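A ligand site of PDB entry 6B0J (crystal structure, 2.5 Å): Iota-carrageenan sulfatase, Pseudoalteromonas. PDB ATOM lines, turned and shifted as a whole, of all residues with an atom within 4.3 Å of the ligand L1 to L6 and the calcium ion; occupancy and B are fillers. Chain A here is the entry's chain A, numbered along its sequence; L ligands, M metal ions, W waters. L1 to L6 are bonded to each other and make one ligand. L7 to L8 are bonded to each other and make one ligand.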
ATOM      1  N   ASP A  11      -6.259  13.144 -17.589  1.00  0.00           N
ATOM      2  CA  ASP A  11      -4.873  12.689 -17.587  1.00  0.00           C
ATOM      3  C   ASP A  11      -4.097  13.326 -18.744  1.00  0.00           C
ATOM      4  O   ASP A  11      -4.364  13.018 -19.902  1.00  0.00           O
ATOM      5  CB  ASP A  11      -4.892  11.149 -17.712  1.00  0.00           C
ATOM      6  CG  ASP A  11      -3.539  10.500 -17.516  1.00  0.00           C
ATOM      7  OD1 ASP A  11      -2.508  11.191 -17.478  1.00  0.00           O
ATOM      8  OD2 ASP A  11      -3.503   9.254 -17.420  1.00  0.00           O
ATOM      9  N   ASP A  12      -3.150  14.207 -18.410  1.00  0.00           N
ATOM     10  CA  ASP A  12      -2.377  15.005 -19.383  1.00  0.00           C
ATOM     11  C   ASP A  12      -3.228  16.055 -20.128  1.00  0.00           C
ATOM     12  O   ASP A  12      -2.877  16.473 -21.254  1.00  0.00           O
ATOM     13  CB  ASP A  12      -1.607  14.128 -20.408  1.00  0.00           C
ATOM     14  CG  ASP A  12      -0.458  13.334 -19.795  1.00  0.00           C
ATOM     15  OD1 ASP A  12      -0.170  13.465 -18.583  1.00  0.00           O
ATOM     16  OD2 ASP A  12       0.190  12.573 -20.532  1.00  0.00           O
ATOM     17  N   PRO A  49       4.536  17.424 -11.306  1.00  0.00           N
ATOM     18  CA  PRO A  49       4.214  17.605 -12.724  1.00  0.00           C
ATOM     19  C   PRO A  49       4.019  16.331 -13.560  1.00  0.00           C
ATOM     20  O   PRO A  49       4.063  16.392 -14.785  1.00  0.00           O
ATOM     21  CB  PRO A  49       5.390  18.436 -13.238  1.00  0.00           C
ATOM     22  CG  PRO A  49       6.541  18.019 -12.377  1.00  0.00           C
ATOM     23  CD  PRO A  49       5.938  17.776 -11.016  1.00  0.00           C
ATOM     24  N   PHE A  50       3.792  15.187 -12.908  1.00  0.00           N
ATOM     25  CA  PHE A  50       3.312  13.988 -13.613  1.00  0.00           C
ATOM     26  C   PHE A  50       2.528  13.033 -12.703  1.00  0.00           C
ATOM     27  O   PHE A  50       2.431  13.255 -11.499  1.00  0.00           O
ATOM     28  CB  PHE A  50       4.418  13.299 -14.424  1.00  0.00           C
ATOM     29  CG  PHE A  50       5.595  12.804 -13.631  1.00  0.00           C
ATOM     30  CD1 PHE A  50       5.501  11.647 -12.894  1.00  0.00           C
ATOM     31  CD2 PHE A  50       6.820  13.458 -13.690  1.00  0.00           C
ATOM     32  CE1 PHE A  50       6.584  11.155 -12.185  1.00  0.00           C
ATOM     33  CE2 PHE A  50       7.929  12.985 -12.986  1.00  0.00           C
ATOM     34  CZ  PHE A  50       7.810  11.831 -12.216  1.00  0.00           C
ATOM     35  N   SER A  51       1.979  11.974 -13.311  1.00  0.00           N
ATOM     36  CA  SER A  51       0.810  11.234 -12.810  1.00  0.00           C
ATOM     37  C   SER A  51       0.837  10.619 -11.425  1.00  0.00           C
ATOM     38  O   SER A  51       0.023  10.980 -10.571  1.00  0.00           O
ATOM     39  CB  SER A  51       0.493  10.111 -13.791  1.00  0.00           C
ATOM     40  OG  SER A  51      -0.584   9.326 -13.357  1.00  0.00           O
ATOM     41  N   ASN A  72       6.889   7.688 -10.801  1.00  0.00           N
ATOM     42  CA  ASN A  72       5.873   6.758 -11.272  1.00  0.00           C
ATOM     43  C   ASN A  72       6.300   5.332 -10.928  1.00  0.00           C
ATOM     44  O   ASN A  72       7.503   5.025 -10.904  1.00  0.00           O
ATOM     45  CB  ASN A  72       5.667   6.863 -12.782  1.00  0.00           C
ATOM     46  CG  ASN A  72       4.867   8.082 -13.201  1.00  0.00           C
ATOM     47  OD1 ASN A  72       4.194   8.718 -12.391  1.00  0.00           O
ATOM     48  ND2 ASN A  72       4.920   8.418 -14.493  1.00  0.00           N
ATOM     49  N   LYS A 105      -8.302   4.983 -14.106  1.00  0.00           N
ATOM     50  CA  LYS A 105      -6.869   4.899 -13.819  1.00  0.00           C
ATOM     51  C   LYS A 105      -6.587   4.947 -12.327  1.00  0.00           C
ATOM     52  O   LYS A 105      -7.120   5.801 -11.628  1.00  0.00           O
ATOM     53  CB  LYS A 105      -6.132   6.050 -14.509  1.00  0.00           C
ATOM     54  CG  LYS A 105      -4.634   6.046 -14.317  1.00  0.00           C
ATOM     55  CD  LYS A 105      -3.941   6.987 -15.295  1.00  0.00           C
ATOM     56  CE  LYS A 105      -2.531   7.287 -14.821  1.00  0.00           C
ATOM     57  NZ  LYS A 105      -1.743   8.096 -15.778  1.00  0.00           N
ATOM     58  N   HIS A 107      -2.889   3.757 -10.828  1.00  0.00           N
ATOM     59  CA  HIS A 107      -1.467   4.185 -10.844  1.00  0.00           C
ATOM     60  C   HIS A 107      -0.905   4.428  -9.440  1.00  0.00           C
ATOM     61  O   HIS A 107      -0.027   5.273  -9.249  1.00  0.00           O
ATOM     62  CB  HIS A 107      -1.305   5.431 -11.748  1.00  0.00           C
ATOM     63  CG  HIS A 107       0.025   5.513 -12.443  1.00  0.00           C
ATOM     64  ND1 HIS A 107       0.516   6.706 -12.949  1.00  0.00           N
ATOM     65  CD2 HIS A 107       0.955   4.569 -12.731  1.00  0.00           C
ATOM     66  CE1 HIS A 107       1.690   6.486 -13.516  1.00  0.00           C
ATOM     67  NE2 HIS A 107       1.976   5.201 -13.406  1.00  0.00           N
ATOM     68  N   GLY A 130      -0.677   2.747 -15.466  1.00  0.00           N
ATOM     69  CA  GLY A 130      -0.479   4.136 -15.880  1.00  0.00           C
ATOM     70  C   GLY A 130      -1.345   4.627 -17.024  1.00  0.00           C
ATOM     71  O   GLY A 130      -1.384   5.817 -17.326  1.00  0.00           O
ATOM     72  N   GLY A 131      -2.040   3.696 -17.678  1.00  0.00           N
ATOM     73  CA  GLY A 131      -2.952   4.040 -18.754  1.00  0.00           C
ATOM     74  C   GLY A 131      -3.509   2.790 -19.390  1.00  0.00           C
ATOM     75  O   GLY A 131      -3.374   1.677 -18.850  1.00  0.00           O
ATOM     76  N   PHE A 155       2.210  -5.949 -21.400  1.00  0.00           N
ATOM     77  CA  PHE A 155       2.040  -4.510 -21.356  1.00  0.00           C
ATOM     78  C   PHE A 155       0.676  -4.162 -20.764  1.00  0.00           C
ATOM     79  O   PHE A 155      -0.355  -4.610 -21.274  1.00  0.00           O
ATOM     80  CB  PHE A 155       2.182  -3.959 -22.784  1.00  0.00           C
ATOM     81  CG  PHE A 155       2.072  -2.464 -22.901  1.00  0.00           C
ATOM     82  CD1 PHE A 155       2.643  -1.609 -21.938  1.00  0.00           C
ATOM     83  CD2 PHE A 155       1.440  -1.907 -24.001  1.00  0.00           C
ATOM     84  CE1 PHE A 155       2.555  -0.239 -22.076  1.00  0.00           C
ATOM     85  CE2 PHE A 155       1.345  -0.530 -24.144  1.00  0.00           C
ATOM     86  CZ  PHE A 155       1.892   0.305 -23.176  1.00  0.00           C
ATOM     87  N   TYR A 157      -1.324  -1.788 -20.692  1.00  0.00           N
ATOM     88  CA  TYR A 157      -2.304  -1.070 -21.520  1.00  0.00           C
ATOM     89  C   TYR A 157      -3.278  -1.955 -22.323  1.00  0.00           C
ATOM     90  O   TYR A 157      -4.316  -1.453 -22.776  1.00  0.00           O
ATOM     91  CB  TYR A 157      -1.596  -0.127 -22.513  1.00  0.00           C
ATOM     92  CG  TYR A 157      -1.150   1.207 -21.938  1.00  0.00           C
ATOM     93  CD1 TYR A 157      -1.570   2.411 -22.527  1.00  0.00           C
ATOM     94  CD2 TYR A 157      -0.308   1.274 -20.825  1.00  0.00           C
ATOM     95  CE1 TYR A 157      -1.167   3.632 -22.021  1.00  0.00           C
ATOM     96  CE2 TYR A 157       0.097   2.492 -20.306  1.00  0.00           C
ATOM     97  CZ  TYR A 157      -0.333   3.664 -20.902  1.00  0.00           C
ATOM     98  OH  TYR A 157       0.058   4.885 -20.403  1.00  0.00           O
ATOM     99  N   HIS A 206      -4.542  11.140 -22.382  1.00  0.00           N
ATOM    100  CA  HIS A 206      -3.197  10.552 -22.338  1.00  0.00           C
ATOM    101  C   HIS A 206      -3.016   9.593 -23.505  1.00  0.00           C
ATOM    102  O   HIS A 206      -3.980   9.014 -23.999  1.00  0.00           O
ATOM    103  CB  HIS A 206      -3.029   9.779 -21.018  1.00  0.00           C
ATOM    104  CG  HIS A 206      -1.640   9.288 -20.746  1.00  0.00           C
ATOM    105  ND1 HIS A 206      -1.095   8.208 -21.382  1.00  0.00           N
ATOM    106  CD2 HIS A 206      -0.729   9.694 -19.830  1.00  0.00           C
ATOM    107  CE1 HIS A 206       0.116   7.982 -20.910  1.00  0.00           C
ATOM    108  NE2 HIS A 206       0.367   8.871 -19.962  1.00  0.00           N
ATOM    109  N   THR A 207      -1.759   9.424 -23.929  1.00  0.00           N
ATOM    110  CA  THR A 207      -1.392   8.466 -24.976  1.00  0.00           C
ATOM    111  C   THR A 207      -1.892   7.040 -24.650  1.00  0.00           C
ATOM    112  O   THR A 207      -2.047   6.707 -23.471  1.00  0.00           O
ATOM    113  CB  THR A 207       0.134   8.421 -25.167  1.00  0.00           C
ATOM    114  OG1 THR A 207       0.753   8.135 -23.911  1.00  0.00           O
ATOM    115  CG2 THR A 207       0.675   9.747 -25.686  1.00  0.00           C
ATOM    116  N   ASP A 264      -4.423  15.889 -13.847  1.00  0.00           N
ATOM    117  CA  ASP A 264      -3.395  15.384 -12.930  1.00  0.00           C
ATOM    118  C   ASP A 264      -2.078  16.125 -13.108  1.00  0.00           C
ATOM    119  O   ASP A 264      -1.296  16.235 -12.169  1.00  0.00           O
ATOM    120  CB  ASP A 264      -3.207  13.858 -13.043  1.00  0.00           C
ATOM    121  CG  ASP A 264      -2.576  13.412 -14.342  1.00  0.00           C
ATOM    122  OD1 ASP A 264      -2.587  14.142 -15.367  1.00  0.00           O
ATOM    123  OD2 ASP A 264      -2.070  12.274 -14.349  1.00  0.00           O
ATOM    124  N   ASN A 265      -1.821  16.603 -14.325  1.00  0.00           N
ATOM    125  CA  ASN A 265      -0.638  17.391 -14.623  1.00  0.00           C
ATOM    126  C   ASN A 265      -0.858  18.192 -15.908  1.00  0.00           C
ATOM    127  O   ASN A 265      -1.919  18.121 -16.549  1.00  0.00           O
ATOM    128  CB  ASN A 265       0.585  16.487 -14.710  1.00  0.00           C
ATOM    129  CG  ASN A 265       0.403  15.333 -15.670  1.00  0.00           C
ATOM    130  OD1 ASN A 265       0.378  14.166 -15.245  1.00  0.00           O
ATOM    131  ND2 ASN A 265       0.283  15.621 -16.957  1.00  0.00           N
ATOM    132  N   LYS A 282       3.996  19.013 -19.565  1.00  0.00           N
ATOM    133  CA  LYS A 282       4.093  17.838 -18.699  1.00  0.00           C
ATOM    134  C   LYS A 282       5.531  17.563 -18.198  1.00  0.00           C
ATOM    135  O   LYS A 282       6.476  17.521 -18.988  1.00  0.00           O
ATOM    136  CB  LYS A 282       3.602  16.602 -19.456  1.00  0.00           C
ATOM    137  CG  LYS A 282       3.427  15.349 -18.603  1.00  0.00           C
ATOM    138  CD  LYS A 282       3.094  14.154 -19.478  1.00  0.00           C
ATOM    139  CE  LYS A 282       3.046  12.875 -18.667  1.00  0.00           C
ATOM    140  NZ  LYS A 282       2.719  11.696 -19.508  1.00  0.00           N
ATOM    141  N   GLY A 283       5.652  17.378 -16.884  1.00  0.00           N
ATOM    142  CA  GLY A 283       6.922  17.041 -16.243  1.00  0.00           C
ATOM    143  C   GLY A 283       7.801  18.214 -15.824  1.00  0.00           C
ATOM    144  O   GLY A 283       8.791  18.006 -15.088  1.00  0.00           O
ATOM    145  N   ARG A 360      10.747  17.896  -8.982  1.00  0.00           N
ATOM    146  CA  ARG A 360      10.751  16.788  -9.928  1.00  0.00           C
ATOM    147  C   ARG A 360      12.184  16.390 -10.189  1.00  0.00           C
ATOM    148  O   ARG A 360      12.986  17.216 -10.605  1.00  0.00           O
ATOM    149  CB  ARG A 360      10.069  17.184 -11.250  1.00  0.00           C
ATOM    150  CG  ARG A 360      10.064  16.078 -12.319  1.00  0.00           C
ATOM    151  CD  ARG A 360      11.182  16.233 -13.347  1.00  0.00           C
ATOM    152  NE  ARG A 360      11.405  15.003 -14.106  1.00  0.00           N
ATOM    153  CZ  ARG A 360      10.659  14.561 -15.124  1.00  0.00           C
ATOM    154  NH1 ARG A 360      10.972  13.425 -15.712  1.00  0.00           N
ATOM    155  NH2 ARG A 360       9.592  15.237 -15.563  1.00  0.00           N
ATOM    156  N   ARG A 362      15.512  14.401 -11.845  1.00  0.00           N
ATOM    157  CA  ARG A 362      16.078  14.069 -13.143  1.00  0.00           C
ATOM    158  C   ARG A 362      17.406  13.325 -12.897  1.00  0.00           C
ATOM    159  O   ARG A 362      17.669  12.906 -11.764  1.00  0.00           O
ATOM    160  CB  ARG A 362      16.224  15.345 -13.972  1.00  0.00           C
ATOM    161  CG  ARG A 362      14.874  15.966 -14.345  1.00  0.00           C
ATOM    162  CD  ARG A 362      14.997  17.056 -15.398  1.00  0.00           C
ATOM    163  NE  ARG A 362      13.717  17.718 -15.664  1.00  0.00           N
ATOM    164  CZ  ARG A 362      12.736  17.275 -16.466  1.00  0.00           C
ATOM    165  NH1 ARG A 362      12.842  16.103 -17.093  1.00  0.00           N
ATOM    166  NH2 ARG A 362      11.629  18.008 -16.628  1.00  0.00           N
ATOM    167  N   LYS A 363      18.202  13.109 -13.946  1.00  0.00           N
ATOM    168  CA  LYS A 363      19.444  12.331 -13.839  1.00  0.00           C
ATOM    169  C   LYS A 363      20.545  13.184 -13.205  1.00  0.00           C
ATOM    170  O   LYS A 363      21.163  14.016 -13.873  1.00  0.00           O
ATOM    171  CB  LYS A 363      19.895  11.788 -15.203  1.00  0.00           C
ATOM    172  CG  LYS A 363      21.049  10.780 -15.119  1.00  0.00           C
ATOM    173  CD  LYS A 363      21.647  10.443 -16.481  1.00  0.00           C
ATOM    174  CE  LYS A 363      20.673   9.651 -17.347  1.00  0.00           C
ATOM    175  NZ  LYS A 363      21.192   9.347 -18.714  1.00  0.00           N
ATOM    176  N   HIS A 429      10.456   4.374 -11.786  1.00  0.00           N
ATOM    177  CA  HIS A 429       9.643   3.879 -12.928  1.00  0.00           C
ATOM    178  C   HIS A 429      10.418   2.908 -13.839  1.00  0.00           C
ATOM    179  O   HIS A 429       9.815   2.153 -14.580  1.00  0.00           O
ATOM    180  CB  HIS A 429       9.007   5.053 -13.715  1.00  0.00           C
ATOM    181  CG  HIS A 429       9.832   5.560 -14.853  1.00  0.00           C
ATOM    182  ND1 HIS A 429      10.992   6.286 -14.664  1.00  0.00           N
ATOM    183  CD2 HIS A 429       9.655   5.489 -16.200  1.00  0.00           C
ATOM    184  CE1 HIS A 429      11.503   6.608 -15.840  1.00  0.00           C
ATOM    185  NE2 HIS A 429      10.701   6.151 -16.789  1.00  0.00           N
ATOM    186  N   GLU A 433      16.895   4.042 -13.766  1.00  0.00           N
ATOM    187  CA  GLU A 433      16.634   5.268 -13.026  1.00  0.00           C
ATOM    188  C   GLU A 433      17.053   5.152 -11.542  1.00  0.00           C
ATOM    189  O   GLU A 433      17.674   6.059 -10.990  1.00  0.00           O
ATOM    190  CB  GLU A 433      15.150   5.648 -13.103  1.00  0.00           C
ATOM    191  CG  GLU A 433      14.844   7.061 -12.655  1.00  0.00           C
ATOM    192  CD  GLU A 433      13.409   7.446 -12.942  1.00  0.00           C
ATOM    193  OE1 GLU A 433      12.515   6.627 -12.646  1.00  0.00           O
ATOM    194  OE2 GLU A 433      13.179   8.572 -13.454  1.00  0.00           O
HETATM  195  C1  LIG L   1       6.763  -0.389 -24.430  1.00  0.00           C
HETATM  196  C2  LIG L   1       6.629   1.125 -24.613  1.00  0.00           C
HETATM  197  C3  LIG L   1       5.184   1.561 -24.827  1.00  0.00           C
HETATM  198  C4  LIG L   1       4.471   0.671 -25.865  1.00  0.00           C
HETATM  199  C5  LIG L   1       4.704  -0.808 -25.536  1.00  0.00           C
HETATM  200  C6  LIG L   1       4.051  -1.748 -26.528  1.00  0.00           C
HETATM  201  O1  LIG L   1       8.157  -0.711 -24.453  1.00  0.00           O
HETATM  202  O2  LIG L   1       7.095   1.809 -23.442  1.00  0.00           O
HETATM  203  O3  LIG L   1       5.210   2.951 -25.215  1.00  0.00           O
HETATM  204  O4  LIG L   1       4.923   0.988 -27.176  1.00  0.00           O
HETATM  205  O5  LIG L   1       6.101  -1.093 -25.476  1.00  0.00           O
HETATM  206  O6  LIG L   1       4.163  -3.081 -26.015  1.00  0.00           O
HETATM  207  S1  LIG L   1       4.025   1.756 -28.176  1.00  0.00           S
HETATM  208  O7  LIG L   1       3.369   2.873 -27.563  1.00  0.00           O
HETATM  209  O8  LIG L   1       4.830   2.233 -29.268  1.00  0.00           O
HETATM  210  O9  LIG L   1       2.857   0.752 -28.681  1.00  0.00           O
HETATM  211  C1  LG2 L   2       4.197   5.151 -25.215  1.00  0.00           C
HETATM  212  C2  LG2 L   2       3.934   6.075 -22.943  1.00  0.00           C
HETATM  213  C3  LG2 L   2       3.287   4.754 -22.610  1.00  0.00           C
HETATM  214  C4  LG2 L   2       1.908   4.888 -23.236  1.00  0.00           C
HETATM  215  O1  LG2 L   2       3.437   7.187 -22.187  1.00  0.00           O
HETATM  216  O2  LG2 L   2       4.075   3.735 -23.219  1.00  0.00           O
HETATM  217  O3  LG2 L   2       2.086   5.797 -24.321  1.00  0.00           O
HETATM  218  C5  LG2 L   2       3.457   6.167 -24.369  1.00  0.00           C
HETATM  219  O4  LG2 L   2       5.552   5.566 -25.285  1.00  0.00           O
HETATM  220  C6  LG2 L   2       4.119   3.723 -24.655  1.00  0.00           C
HETATM  221  C1  LG3 L   3       3.888   7.158 -20.830  1.00  0.00           C
HETATM  222  C2  LG3 L   3       4.379   8.536 -20.431  1.00  0.00           C
HETATM  223  C3  LG3 L   3       4.802   8.515 -18.974  1.00  0.00           C
HETATM  224  C4  LG3 L   3       3.633   8.079 -18.097  1.00  0.00           C
HETATM  225  C5  LG3 L   3       3.221   6.689 -18.602  1.00  0.00           C
HETATM  226  C6  LG3 L   3       2.072   6.086 -17.816  1.00  0.00           C
HETATM  227  O1  LG3 L   3       5.466   8.920 -21.277  1.00  0.00           O
HETATM  228  O2  LG3 L   3       5.298   9.807 -18.570  1.00  0.00           O
HETATM  229  O3  LG3 L   3       2.561   9.039 -18.099  1.00  0.00           O
HETATM  230  O4  LG3 L   3       2.843   6.762 -19.970  1.00  0.00           O
HETATM  231  O5  LG3 L   3       1.913   4.761 -18.302  1.00  0.00           O
HETATM  232  S1  LG3 L   3       2.037   9.585 -16.763  1.00  0.00           S
HETATM  233  O6  LG3 L   3       0.909  10.745 -16.927  1.00  0.00           O
HETATM  234  O7  LG3 L   3       3.109  10.191 -16.046  1.00  0.00           O
HETATM  235  O8  LG3 L   3       1.525   8.483 -16.040  1.00  0.00           O
HETATM  236  C1  LG4 L   4       6.432   9.690 -17.692  1.00  0.00           C
HETATM  237  C2  LG4 L   4       6.822  11.070 -17.172  1.00  0.00           C
HETATM  238  C3  LG4 L   4       8.203  11.009 -16.498  1.00  0.00           C
HETATM  239  C4  LG4 L   4       9.249  10.470 -17.469  1.00  0.00           C
HETATM  240  C5  LG4 L   4       8.766   9.051 -17.511  1.00  0.00           C
HETATM  241  C6  LG4 L   4       8.533   8.778 -16.028  1.00  0.00           C
HETATM  242  O1  LG4 L   4       6.785  11.961 -18.284  1.00  0.00           O
HETATM  243  O2  LG4 L   4       8.137  10.046 -15.454  1.00  0.00           O
HETATM  244  O3  LG4 L   4      10.589  10.531 -16.971  1.00  0.00           O
HETATM  245  O4  LG4 L   4       7.575   9.042 -18.298  1.00  0.00           O
HETATM  246  O5  LG4 L   4       6.437  14.155 -19.313  1.00  0.00           O
HETATM  247  O6  LG4 L   4       8.430  13.768 -18.159  1.00  0.00           O
HETATM  248  O7  LG4 L   4       6.369  14.033 -16.807  1.00  0.00           O
HETATM  249  S1  LG4 L   4       7.016  13.490 -18.185  1.00  0.00           S
HETATM  250  C1  LG5 L   5      11.573  10.303 -17.999  1.00  0.00           C
HETATM  251  C2  LG5 L   5      12.306  11.608 -18.294  1.00  0.00           C
HETATM  252  C3  LG5 L   5      13.519  11.396 -19.195  1.00  0.00           C
HETATM  253  C4  LG5 L   5      14.383  10.246 -18.647  1.00  0.00           C
HETATM  254  C5  LG5 L   5      13.551   8.982 -18.463  1.00  0.00           C
HETATM  255  C6  LG5 L   5      14.369   7.794 -17.927  1.00  0.00           C
HETATM  256  O1  LG5 L   5      11.428  12.564 -18.907  1.00  0.00           O
HETATM  257  O2  LG5 L   5      14.211  12.655 -19.321  1.00  0.00           O
HETATM  258  O3  LG5 L   5      14.960  10.579 -17.368  1.00  0.00           O
HETATM  259  O4  LG5 L   5      12.481   9.282 -17.561  1.00  0.00           O
HETATM  260  O5  LG5 L   5      13.687   6.566 -18.191  1.00  0.00           O
HETATM  261  S1  LG5 L   5      16.485  10.588 -17.073  1.00  0.00           S
HETATM  262  O6  LG5 L   5      16.697  10.103 -15.526  1.00  0.00           O
HETATM  263  O7  LG5 L   5      16.994  11.936 -17.230  1.00  0.00           O
HETATM  264  O8  LG5 L   5      17.180   9.681 -17.928  1.00  0.00           O
HETATM  265  C1  LG6 L   6      15.998  13.857 -20.552  1.00  0.00           C
HETATM  266  C2  LG6 L   6      15.438  14.636 -22.852  1.00  0.00           C
HETATM  267  C3  LG6 L   6      14.688  13.327 -22.998  1.00  0.00           C
HETATM  268  C4  LG6 L   6      15.823  12.350 -23.308  1.00  0.00           C
HETATM  269  O1  LG6 L   6      15.972  15.136 -24.071  1.00  0.00           O
HETATM  270  O2  LG6 L   6      14.016  13.056 -21.747  1.00  0.00           O
HETATM  271  O3  LG6 L   6      16.965  12.893 -22.593  1.00  0.00           O
HETATM  272  C5  LG6 L   6      16.557  14.121 -21.955  1.00  0.00           C
HETATM  273  O4  LG6 L   6      15.509  15.076 -19.989  1.00  0.00           O
HETATM  274  C6  LG6 L   6      14.890  12.790 -20.609  1.00  0.00           C
HETATM  275  C1  LG7 L   7       2.798   4.743 -32.917  1.00  0.00           C
HETATM  276  C2  LG7 L   7       4.001   5.536 -32.399  1.00  0.00           C
HETATM  277  C3  LG7 L   7       4.370   5.095 -30.982  1.00  0.00           C
HETATM  278  C4  LG7 L   7       3.147   5.161 -30.053  1.00  0.00           C
HETATM  279  C5  LG7 L   7       1.966   4.380 -30.680  1.00  0.00           C
HETATM  280  C6  LG7 L   7       0.687   4.473 -29.848  1.00  0.00           C
HETATM  281  O1  LG7 L   7       2.379   5.221 -34.209  1.00  0.00           O
HETATM  282  O2  LG7 L   7       5.126   5.345 -33.271  1.00  0.00           O
HETATM  283  O3  LG7 L   7       5.454   5.904 -30.484  1.00  0.00           O
HETATM  284  O4  LG7 L   7       2.808   6.531 -29.737  1.00  0.00           O
HETATM  285  O5  LG7 L   7       1.693   4.855 -32.011  1.00  0.00           O
HETATM  286  O6  LG7 L   7      -0.379   3.712 -30.409  1.00  0.00           O
HETATM  287  S1  LG7 L   7       2.463   7.080 -28.331  1.00  0.00           S
HETATM  288  O7  LG7 L   7       3.662   7.261 -27.557  1.00  0.00           O
HETATM  289  O8  LG7 L   7       1.801   8.348 -28.493  1.00  0.00           O
HETATM  290  O9  LG7 L   7       1.440   6.109 -27.495  1.00  0.00           O
HETATM  291  C1  LG8 L   8       6.243   5.244 -29.458  1.00  0.00           C
HETATM  292  C2  LG8 L   8       7.051   6.293 -28.652  1.00  0.00           C
HETATM  293  C3  LG8 L   8       8.308   5.683 -28.016  1.00  0.00           C
HETATM  294  C4  LG8 L   8       9.102   4.999 -29.109  1.00  0.00           C
HETATM  295  C5  LG8 L   8       8.212   3.772 -29.225  1.00  0.00           C
HETATM  296  C6  LG8 L   8       7.844   3.422 -27.778  1.00  0.00           C
HETATM  297  O1  LG8 L   8       7.405   7.419 -29.477  1.00  0.00           O
HETATM  298  O2  LG8 L   8       7.913   4.670 -27.082  1.00  0.00           O
HETATM  299  O3  LG8 L   8      10.481   4.736 -28.761  1.00  0.00           O
HETATM  300  O4  LG8 L   8       7.046   4.143 -29.986  1.00  0.00           O
HETATM  301  O5  LG8 L   8       6.985   9.131 -27.787  1.00  0.00           O
HETATM  302  O6  LG8 L   8       7.791   9.795 -29.896  1.00  0.00           O
HETATM  303  O7  LG8 L   8       9.397   8.685 -28.350  1.00  0.00           O
HETATM  304  S1  LG8 L   8       7.856   8.773 -28.882  1.00  0.00           S
HETATM  305 CA    CA M   1      -0.739  12.368 -16.557  1.00  0.00          CA
HETATM  306  O   HOH W   1       5.293  11.938 -20.816  1.00  0.00           O
HETATM  307  O   HOH W   2      10.709  15.456 -19.268  1.00  0.00           O
HETATM  308  O   HOH W   3       8.801   8.634 -12.953  1.00  0.00           O
HETATM  309  O   HOH W   4      14.880  10.518 -13.482  1.00  0.00           O
HETATM  310  O   HOH W   5       4.824  10.235 -23.409  1.00  0.00           O
HETATM  311  O   HOH W   6      10.974   9.728 -13.761  1.00  0.00           O
HETATM  312  O   HOH W   7       7.700  13.734 -21.645  1.00  0.00           O
HETATM  313  O   HOH W   8      18.101   8.668 -13.787  1.00  0.00           O
HETATM  314  O   HOH W   9      13.467  12.340 -14.888  1.00  0.00           O
HETATM  315  O   HOH W  10       5.823   6.077 -16.263  1.00  0.00           O
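O5 of LG5 L5 sits close to NE2 of His 429 (3.3 Å).
NZ of Lys 282 is in salt-bridge range of O7 of LG3 L3 (3.8 Å).
The side-chain amide nitrogen (ND2) of Asn 72 sits at hydrogen-bond distance from an oxygen (O7) of LG3 L3, at 3.0 Å.
An oxygen (O3) of LG3 L3 lies within hydrogen-bond range of a ring nitrogen (NE2) of His 206 (2.9 Å).
O8 of LG3 L3 lies within salt-bridge range of NZ of Lys 105 (3.3 Å).
O7 of LG4 L4 sits close to N of Gly 283 (3.4 Å).
The guanidinium group (NH2) of Arg 360 is in salt-bridge range of an oxygen (O6) of LG4 L4.
The backbone NH (N) of Ser 51 lies close to an oxygen (O7) of LG3 L3, 3.5 Å away.
The side-chain hydroxyl (OG1) of Thr 207 lies within hydrogen-bond range of an oxygen (O3) of LG2 L2 (2.7 Å).
OH of Tyr 157 is in hydrogen-bond range of O5 of LG3 L3.
An oxygen (O4) of LG2 L2 is in hydrogen-bond range of an oxygen (O2) of LG8 L8.
OG of Ser 51 lies within hydrogen-bond range of NZ of Lys 105 (3.0 Å).
The side-chain amino group (NZ) of Lys 282 lies within salt-bridge range of the side-chain carboxylate (OD2) of Asp 12.
The guanidinium group (NH2) of Arg 362 lies within hydrogen-bond range of the backbone carbonyl oxygen (O) of Gly 283 (3.2 Å).
The side-chain carboxylate (OE1) of Glu 433 sits at hydrogen-bond distance from a ring nitrogen (ND1) of His 429 (2.6 Å).
A ring nitrogen (ND1) of His 107 lies within hydrogen-bond range of the side-chain hydroxyl (OG) of Ser 51 (2.9 Å).
N of Ser 51 sits close to OD1 of Asn 265 (3.3 Å).
The backbone NH (N) of Gly 283 sits at hydrogen-bond distance from the backbone carbonyl oxygen (O) of Pro 49, at 2.8 Å.
The backbone carbonyl oxygen (O) of Gly 283 sits at hydrogen-bond distance from the guanidinium group (NH2) of Arg 360.
Pro 49 touches the ligand L1 to L6.
CB of Phe 50 touches O7 of LG4 L4, 3.2 Å away.
His 107 touches the ligand L1 to L6.
CA of Gly 130 touches O5 of LG3 L3, at 3.5 Å.
CD2 of Phe 155 touches O6 of LIG L1, at 3.6 Å.
CE of Lys 363 touches O8 of LG5 L5, 3.5 Å away.
Hydrophobic or aromatic side chains that line the ligand L1 to L6: Phe 50, His 107, Phe 155, Tyr 157, His 206 and His 429.
The nearest printed residue that does not touch the ligand L1 to L6 is Arg 362 (4.1 Å).
Merely in contact with the calcium ion: Ser 51 (3.8 Å).
Within 4 Å of the calcium ion: Asp 11, Asp 12, Ser 51, Asp 264 and Asn 265.
The calcium ion is bound by OD1 of Asp 11 (2.3 Å), O6 of LG3 L3 (2.3 Å), OD1 of Asp 12 (2.4 Å), OD1 of Asn 265 (2.5 Å), OD2 of Asp 264 (2.6 Å) and OD1 of Asp 264 (2.8 Å).
The calcium ion has six donor atoms within binding distance.
Water W4 lies within hydrogen-bond range of the side-chain carboxylate of Glu 433 (2.6 Å) and an oxygen (O6) of LG5 L5 (2.8 Å).
Water W1 lies within hydrogen-bond range of NZ of Lys 282 (2.9 Å) and O5 of LG4 L4 (2.9 Å).
Water W3 bridges an oxygen (O2) of LG4 L4 (2.9 Å) and the backbone NH (N) of Asn 72 (3.0 Å).
Water W2 bridges an oxygen (O1) of LG5 L5 (3.0 Å) and the guanidinium group (NH1) of Arg 362 (3.1 Å).
Water W6 lies within hydrogen-bond range of the side-chain carboxylate of Glu 433 and an oxygen (O2) of LG4 L4.
Water W9 lies within hydrogen-bond range of NH1 of Arg 360 (2.8 Å) and O3 of LG5 L5 (3.4 Å).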
